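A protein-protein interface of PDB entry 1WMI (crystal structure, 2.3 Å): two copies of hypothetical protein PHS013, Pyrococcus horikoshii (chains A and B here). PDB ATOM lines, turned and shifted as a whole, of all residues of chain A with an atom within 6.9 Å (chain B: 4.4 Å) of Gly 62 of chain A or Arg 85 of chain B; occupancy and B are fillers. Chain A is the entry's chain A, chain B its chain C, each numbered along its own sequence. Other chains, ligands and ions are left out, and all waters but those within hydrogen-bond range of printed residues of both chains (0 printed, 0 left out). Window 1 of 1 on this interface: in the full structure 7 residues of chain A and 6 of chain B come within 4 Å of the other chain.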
ATOM      1  N   HIS A  22      10.650  26.507  19.917  1.00  0.00           N
ATOM      2  CA  HIS A  22      10.266  27.052  18.617  1.00  0.00           C
ATOM      3  C   HIS A  22       9.974  28.548  18.687  1.00  0.00           C
ATOM      4  O   HIS A  22      10.291  29.304  17.765  1.00  0.00           O
ATOM      5  CB  HIS A  22       9.036  26.322  18.080  1.00  0.00           C
ATOM      6  CG  HIS A  22       9.301  24.902  17.681  1.00  0.00           C
ATOM      7  ND1 HIS A  22       9.733  23.946  18.580  1.00  0.00           N
ATOM      8  CD2 HIS A  22       9.193  24.283  16.488  1.00  0.00           C
ATOM      9  CE1 HIS A  22       9.875  22.795  17.946  1.00  0.00           C
ATOM     10  NE2 HIS A  22       9.557  22.967  16.680  1.00  0.00           N
ATOM     11  N   ARG A  25      13.093  30.575  18.654  1.00  0.00           N
ATOM     12  CA  ARG A  25      13.644  30.634  17.301  1.00  0.00           C
ATOM     13  C   ARG A  25      12.950  31.735  16.497  1.00  0.00           C
ATOM     14  O   ARG A  25      13.574  32.435  15.687  1.00  0.00           O
ATOM     15  CB  ARG A  25      13.445  29.274  16.612  1.00  0.00           C
ATOM     16  CG  ARG A  25      14.518  28.900  15.586  1.00  0.00           C
ATOM     17  CD  ARG A  25      14.175  27.570  14.919  1.00  0.00           C
ATOM     18  NE  ARG A  25      13.874  26.531  15.904  1.00  0.00           N
ATOM     19  CZ  ARG A  25      14.785  25.786  16.522  1.00  0.00           C
ATOM     20  NH1 ARG A  25      14.411  24.870  17.411  1.00  0.00           N
ATOM     21  NH2 ARG A  25      16.067  25.940  16.236  1.00  0.00           N
ATOM     22  N   PHE A  43      17.917  31.004   7.033  1.00  0.00           N
ATOM     23  CA  PHE A  43      16.528  30.582   7.064  1.00  0.00           C
ATOM     24  C   PHE A  43      15.965  30.038   5.758  1.00  0.00           C
ATOM     25  O   PHE A  43      14.748  30.032   5.561  1.00  0.00           O
ATOM     26  CB  PHE A  43      15.667  31.734   7.576  1.00  0.00           C
ATOM     27  CG  PHE A  43      15.919  32.074   9.012  1.00  0.00           C
ATOM     28  CD1 PHE A  43      15.467  31.233  10.022  1.00  0.00           C
ATOM     29  CD2 PHE A  43      16.633  33.216   9.359  1.00  0.00           C
ATOM     30  CE1 PHE A  43      15.719  31.517  11.359  1.00  0.00           C
ATOM     31  CE2 PHE A  43      16.891  33.512  10.694  1.00  0.00           C
ATOM     32  CZ  PHE A  43      16.431  32.658  11.697  1.00  0.00           C
ATOM     33  N   ALA A  59      10.133  31.863   4.749  1.00  0.00           N
ATOM     34  CA  ALA A  59      11.277  31.484   5.558  1.00  0.00           C
ATOM     35  C   ALA A  59      10.978  30.158   6.226  1.00  0.00           C
ATOM     36  O   ALA A  59       9.833  29.870   6.582  1.00  0.00           O
ATOM     37  CB  ALA A  59      11.560  32.542   6.607  1.00  0.00           C
ATOM     38  N   ARG A  60      12.017  29.349   6.384  1.00  0.00           N
ATOM     39  CA  ARG A  60      11.876  28.052   7.018  1.00  0.00           C
ATOM     40  C   ARG A  60      12.547  28.104   8.396  1.00  0.00           C
ATOM     41  O   ARG A  60      13.746  28.391   8.517  1.00  0.00           O
ATOM     42  CB  ARG A  60      12.503  26.970   6.124  1.00  0.00           C
ATOM     43  CG  ARG A  60      12.214  25.542   6.563  1.00  0.00           C
ATOM     44  CD  ARG A  60      12.720  24.525   5.545  1.00  0.00           C
ATOM     45  NE  ARG A  60      11.927  24.522   4.317  1.00  0.00           N
ATOM     46  CZ  ARG A  60      10.652  24.143   4.243  1.00  0.00           C
ATOM     47  NH1 ARG A  60      10.017  24.171   3.077  1.00  0.00           N
ATOM     48  NH2 ARG A  60      10.008  23.730   5.330  1.00  0.00           N
ATOM     49  N   LEU A  61      11.762  27.860   9.441  1.00  0.00           N
ATOM     50  CA  LEU A  61      12.300  27.878  10.790  1.00  0.00           C
ATOM     51  C   LEU A  61      12.462  26.467  11.344  1.00  0.00           C
ATOM     52  O   LEU A  61      12.749  26.280  12.523  1.00  0.00           O
ATOM     53  CB  LEU A  61      11.401  28.712  11.709  1.00  0.00           C
ATOM     54  CG  LEU A  61      11.641  30.229  11.698  1.00  0.00           C
ATOM     55  CD1 LEU A  61      11.378  30.808  10.315  1.00  0.00           C
ATOM     56  CD2 LEU A  61      10.744  30.884  12.727  1.00  0.00           C
ATOM     57  N   GLY A  62      12.290  25.473  10.480  1.00  0.00           N
ATOM     58  CA  GLY A  62      12.418  24.091  10.911  1.00  0.00           C
ATOM     59  C   GLY A  62      11.100  23.345  10.809  1.00  0.00           C
ATOM     60  O   GLY A  62      10.685  22.949   9.717  1.00  0.00           O
ATOM     61  N   ASP A  63      10.432  23.168  11.944  1.00  0.00           N
ATOM     62  CA  ASP A  63       9.160  22.458  11.980  1.00  0.00           C
ATOM     63  C   ASP A  63       8.025  23.201  11.284  1.00  0.00           C
ATOM     64  O   ASP A  63       6.937  22.649  11.093  1.00  0.00           O
ATOM     65  CB  ASP A  63       8.757  22.153  13.424  1.00  0.00           C
ATOM     66  CG  ASP A  63       9.774  21.283  14.141  1.00  0.00           C
ATOM     67  OD1 ASP A  63       9.588  21.000  15.342  1.00  0.00           O
ATOM     68  OD2 ASP A  63      10.764  20.882  13.508  1.00  0.00           O
ATOM     69  N   TYR A  64       8.271  24.448  10.900  1.00  0.00           N
ATOM     70  CA  TYR A  64       7.244  25.228  10.229  1.00  0.00           C
ATOM     71  C   TYR A  64       7.845  26.301   9.332  1.00  0.00           C
ATOM     72  O   TYR A  64       9.052  26.528   9.343  1.00  0.00           O
ATOM     73  CB  TYR A  64       6.298  25.856  11.260  1.00  0.00           C
ATOM     74  CG  TYR A  64       6.952  26.864  12.177  1.00  0.00           C
ATOM     75  CD1 TYR A  64       6.861  28.235  11.920  1.00  0.00           C
ATOM     76  CD2 TYR A  64       7.668  26.448  13.304  1.00  0.00           C
ATOM     77  CE1 TYR A  64       7.471  29.172  12.764  1.00  0.00           C
ATOM     78  CE2 TYR A  64       8.282  27.376  14.151  1.00  0.00           C
ATOM     79  CZ  TYR A  64       8.179  28.734  13.875  1.00  0.00           C
ATOM     80  OH  TYR A  64       8.801  29.646  14.703  1.00  0.00           O
ATOM     81  N   ARG A  65       6.989  26.943   8.547  1.00  0.00           N
ATOM     82  CA  ARG A  65       7.412  27.994   7.628  1.00  0.00           C
ATOM     83  C   ARG A  65       6.664  29.297   7.893  1.00  0.00           C
ATOM     84  O   ARG A  65       5.492  29.285   8.286  1.00  0.00           O
ATOM     85  CB  ARG A  65       7.157  27.556   6.186  1.00  0.00           C
ATOM     86  CG  ARG A  65       8.000  26.374   5.724  1.00  0.00           C
ATOM     87  CD  ARG A  65       7.486  25.830   4.404  1.00  0.00           C
ATOM     88  NE  ARG A  65       6.183  25.193   4.570  1.00  0.00           N
ATOM     89  CZ  ARG A  65       5.310  24.999   3.588  1.00  0.00           C
ATOM     90  NH1 ARG A  65       4.149  24.405   3.841  1.00  0.00           N
ATOM     91  NH2 ARG A  65       5.588  25.411   2.358  1.00  0.00           N
ATOM     92  N   PRO A  84       2.792  24.572   7.846  1.00  0.00           N
ATOM     93  CA  PRO A  84       3.392  23.320   8.317  1.00  0.00           C
ATOM     94  C   PRO A  84       4.786  23.105   7.742  1.00  0.00           C
ATOM     95  O   PRO A  84       5.257  23.897   6.933  1.00  0.00           O
ATOM     96  CB  PRO A  84       2.408  22.259   7.824  1.00  0.00           C
ATOM     97  CG  PRO A  84       1.114  22.976   7.820  1.00  0.00           C
ATOM     98  CD  PRO A  84       1.485  24.310   7.219  1.00  0.00           C
ATOM     99  N   ARG A  85       5.429  22.023   8.169  1.00  0.00           N
ATOM    100  CA  ARG A  85       6.768  21.651   7.715  1.00  0.00           C
ATOM    101  C   ARG A  85       6.790  21.736   6.196  1.00  0.00           C
ATOM    102  O   ARG A  85       7.789  22.139   5.578  1.00  0.00           O
ATOM    103  CB  ARG A  85       7.058  20.199   8.102  1.00  0.00           C
ATOM    104  CG  ARG A  85       8.482  19.914   8.529  1.00  0.00           C
ATOM    105  CD  ARG A  85       8.665  20.277   9.985  1.00  0.00           C
ATOM    106  NE  ARG A  85       8.772  19.115  10.867  1.00  0.00           N
ATOM    107  CZ  ARG A  85       9.847  18.838  11.599  1.00  0.00           C
ATOM    108  NH1 ARG A  85      10.903  19.638  11.548  1.00  0.00           N
ATOM    109  NH2 ARG A  85       9.868  17.770  12.382  1.00  0.00           N
ATOM    110  N   GLY A  86       5.648  21.361   5.628  1.00  0.00           N
ATOM    111  CA  GLY A  86       5.448  21.298   4.194  1.00  0.00           C
ATOM    112  C   GLY A  86       5.190  19.816   4.107  1.00  0.00           C
ATOM    113  O   GLY A  86       6.133  19.015   4.171  1.00  0.00           O
ATOM    114  N   ARG B  60      16.148  19.048  -0.347  1.00  0.00           N
ATOM    115  CA  ARG B  60      15.563  18.596   0.910  1.00  0.00           C
ATOM    116  C   ARG B  60      14.523  17.518   0.606  1.00  0.00           C
ATOM    117  O   ARG B  60      13.644  17.707  -0.229  1.00  0.00           O
ATOM    118  CB  ARG B  60      14.893  19.754   1.647  1.00  0.00           C
ATOM    119  CG  ARG B  60      15.851  20.776   2.207  1.00  0.00           C
ATOM    120  CD  ARG B  60      15.105  21.890   2.932  1.00  0.00           C
ATOM    121  NE  ARG B  60      16.010  22.759   3.684  1.00  0.00           N
ATOM    122  CZ  ARG B  60      16.685  22.384   4.769  1.00  0.00           C
ATOM    123  NH1 ARG B  60      17.485  23.247   5.380  1.00  0.00           N
ATOM    124  NH2 ARG B  60      16.556  21.152   5.250  1.00  0.00           N
ATOM    125  N   ASP B  63      12.957  15.342   6.328  1.00  0.00           N
ATOM    126  CA  ASP B  63      13.881  15.583   7.408  1.00  0.00           C
ATOM    127  C   ASP B  63      15.288  15.088   7.156  1.00  0.00           C
ATOM    128  O   ASP B  63      15.894  14.472   8.025  1.00  0.00           O
ATOM    129  CB  ASP B  63      13.312  15.027   8.718  1.00  0.00           C
ATOM    130  CG  ASP B  63      12.154  15.866   9.241  1.00  0.00           C
ATOM    131  OD1 ASP B  63      12.355  17.071   9.518  1.00  0.00           O
ATOM    132  OD2 ASP B  63      11.042  15.314   9.381  1.00  0.00           O
ATOM    133  N   ARG B  65      18.678  16.058   3.988  1.00  0.00           N
ATOM    134  CA  ARG B  65      19.105  16.755   2.788  1.00  0.00           C
ATOM    135  C   ARG B  65      19.869  15.840   1.862  1.00  0.00           C
ATOM    136  O   ARG B  65      20.516  14.889   2.299  1.00  0.00           O
ATOM    137  CB  ARG B  65      19.984  17.949   3.169  1.00  0.00           C
ATOM    138  CG  ARG B  65      19.219  19.141   3.749  1.00  0.00           C
ATOM    139  CD  ARG B  65      20.170  20.198   4.291  1.00  0.00           C
ATOM    140  NE  ARG B  65      20.859  19.714   5.484  1.00  0.00           N
ATOM    141  CZ  ARG B  65      22.084  20.082   5.848  1.00  0.00           C
ATOM    142  NH1 ARG B  65      22.774  20.946   5.115  1.00  0.00           N
ATOM    143  NH2 ARG B  65      22.625  19.574   6.943  1.00  0.00           N
ATOM    144  N   PRO B  84      21.508  15.164   7.564  1.00  0.00           N
ATOM    145  CA  PRO B  84      20.458  15.336   8.587  1.00  0.00           C
ATOM    146  C   PRO B  84      19.565  16.563   8.396  1.00  0.00           C
ATOM    147  O   PRO B  84      19.537  17.142   7.309  1.00  0.00           O
ATOM    148  CB  PRO B  84      21.265  15.442   9.867  1.00  0.00           C
ATOM    149  CG  PRO B  84      22.307  14.460   9.624  1.00  0.00           C
ATOM    150  CD  PRO B  84      22.788  14.862   8.229  1.00  0.00           C
ATOM    151  N   ARG B  85      18.826  16.948   9.445  1.00  0.00           N
ATOM    152  CA  ARG B  85      17.970  18.134   9.363  1.00  0.00           C
ATOM    153  C   ARG B  85      19.028  19.199   9.125  1.00  0.00           C
ATOM    154  O   ARG B  85      18.848  20.096   8.300  1.00  0.00           O
ATOM    155  CB  ARG B  85      17.167  18.357  10.661  1.00  0.00           C
ATOM    156  CG  ARG B  85      17.665  19.434  11.629  1.00  0.00           C
ATOM    157  CD  ARG B  85      16.525  20.405  12.018  1.00  0.00           C
ATOM    158  NE  ARG B  85      16.149  20.386  13.438  1.00  0.00           N
ATOM    159  CZ  ARG B  85      15.151  21.104  13.959  1.00  0.00           C
ATOM    160  NH1 ARG B  85      14.421  21.897  13.182  1.00  0.00           N
ATOM    161  NH2 ARG B  85      14.885  21.044  15.260  1.00  0.00           N
ATOM    162  N   GLY B  86      20.151  19.111   9.833  1.00  0.00           N
ATOM    163  CA  GLY B  86      21.209  20.047   9.494  1.00  0.00           C
ATOM    164  C   GLY B  86      21.893  21.097  10.342  1.00  0.00           C
ATOM    165  O   GLY B  86      22.928  21.616   9.923  1.00  0.00           O
ATOM    166  N   ARG B  87      21.371  21.475  11.490  1.00  0.00           N
ATOM    167  CA  ARG B  87      22.130  22.471  12.216  1.00  0.00           C
ATOM    168  C   ARG B  87      23.214  21.577  12.799  1.00  0.00           C
ATOM    169  O   ARG B  87      23.443  20.484  12.274  1.00  0.00           O
ATOM    170  CB  ARG B  87      21.275  23.111  13.294  1.00  0.00           C
ATOM    171  CG  ARG B  87      20.005  23.796  12.763  1.00  0.00           C
ATOM    172  CD  ARG B  87      19.446  24.659  13.850  1.00  0.00           C
ATOM    173  NE  ARG B  87      19.877  24.108  15.124  1.00  0.00           N
ATOM    174  CZ  ARG B  87      19.214  24.216  16.259  1.00  0.00           C
ATOM    175  NH1 ARG B  87      18.069  24.869  16.302  1.00  0.00           N
ATOM    176  NH2 ARG B  87      19.698  23.630  17.339  1.00  0.00           N
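The guanidinium group (NH1) of Arg 85 of chain B is in salt-bridge range of the side-chain carboxylate (OD2) of Asp 63 of chain A (3.8 Å).
NH1 of Arg 87 of chain B lies close to NH2 of Arg 25 of chain A, at 2.3 Å.
OD1 of Asp 63 of chain B is in salt-bridge range of NH1 of Arg 85 of chain A.
The guanidinium group of Arg 60 of chain A sits at hydrogen-bond distance from the backbone carbonyl oxygen of Arg 85 of chain A, 2.7 Å away.
The backbone carbonyl oxygen (O) of Arg 85 of chain B sits at hydrogen-bond distance from the guanidinium group (NE) of Arg 65 of chain B (3.5 Å).
The guanidinium group of Arg 85 of chain A is in salt-bridge range of the side-chain carboxylate of Asp 63 of chain A (3.4 Å).
Among the printed residues, pairs that only touch across the chains: Gly 62 of chain A with Arg 85 of chain B.
Gly 62 of chain A touches just one residue of chain B: Arg 85 (3.7 Å).
Arg 85 of chain B touches just these residues of chain A: Gly 62 (3.7 Å) and Asp 63 (3.8 Å).
Of the printed residues of chain A, Asp 63 of chain B touches Arg 85 (3.6 Å).
Printed residues of chain B within 4 Å of Asp 63 of chain A: Arg 85 (3.8 Å).
Of the 7 printed residues of chain B, 3 touch a printed residue of chain A.
Of the 13 printed residues of chain A, 4 touch a printed residue of chain B.
Among the printed residues, 4 pairs touch across the chains.
Asp 63 of chain A touches Arg 85 of chain B, and with the chains exchanged Arg 85 of chain A touches Asp 63 of chain B.
6 positions are printed for both chains.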
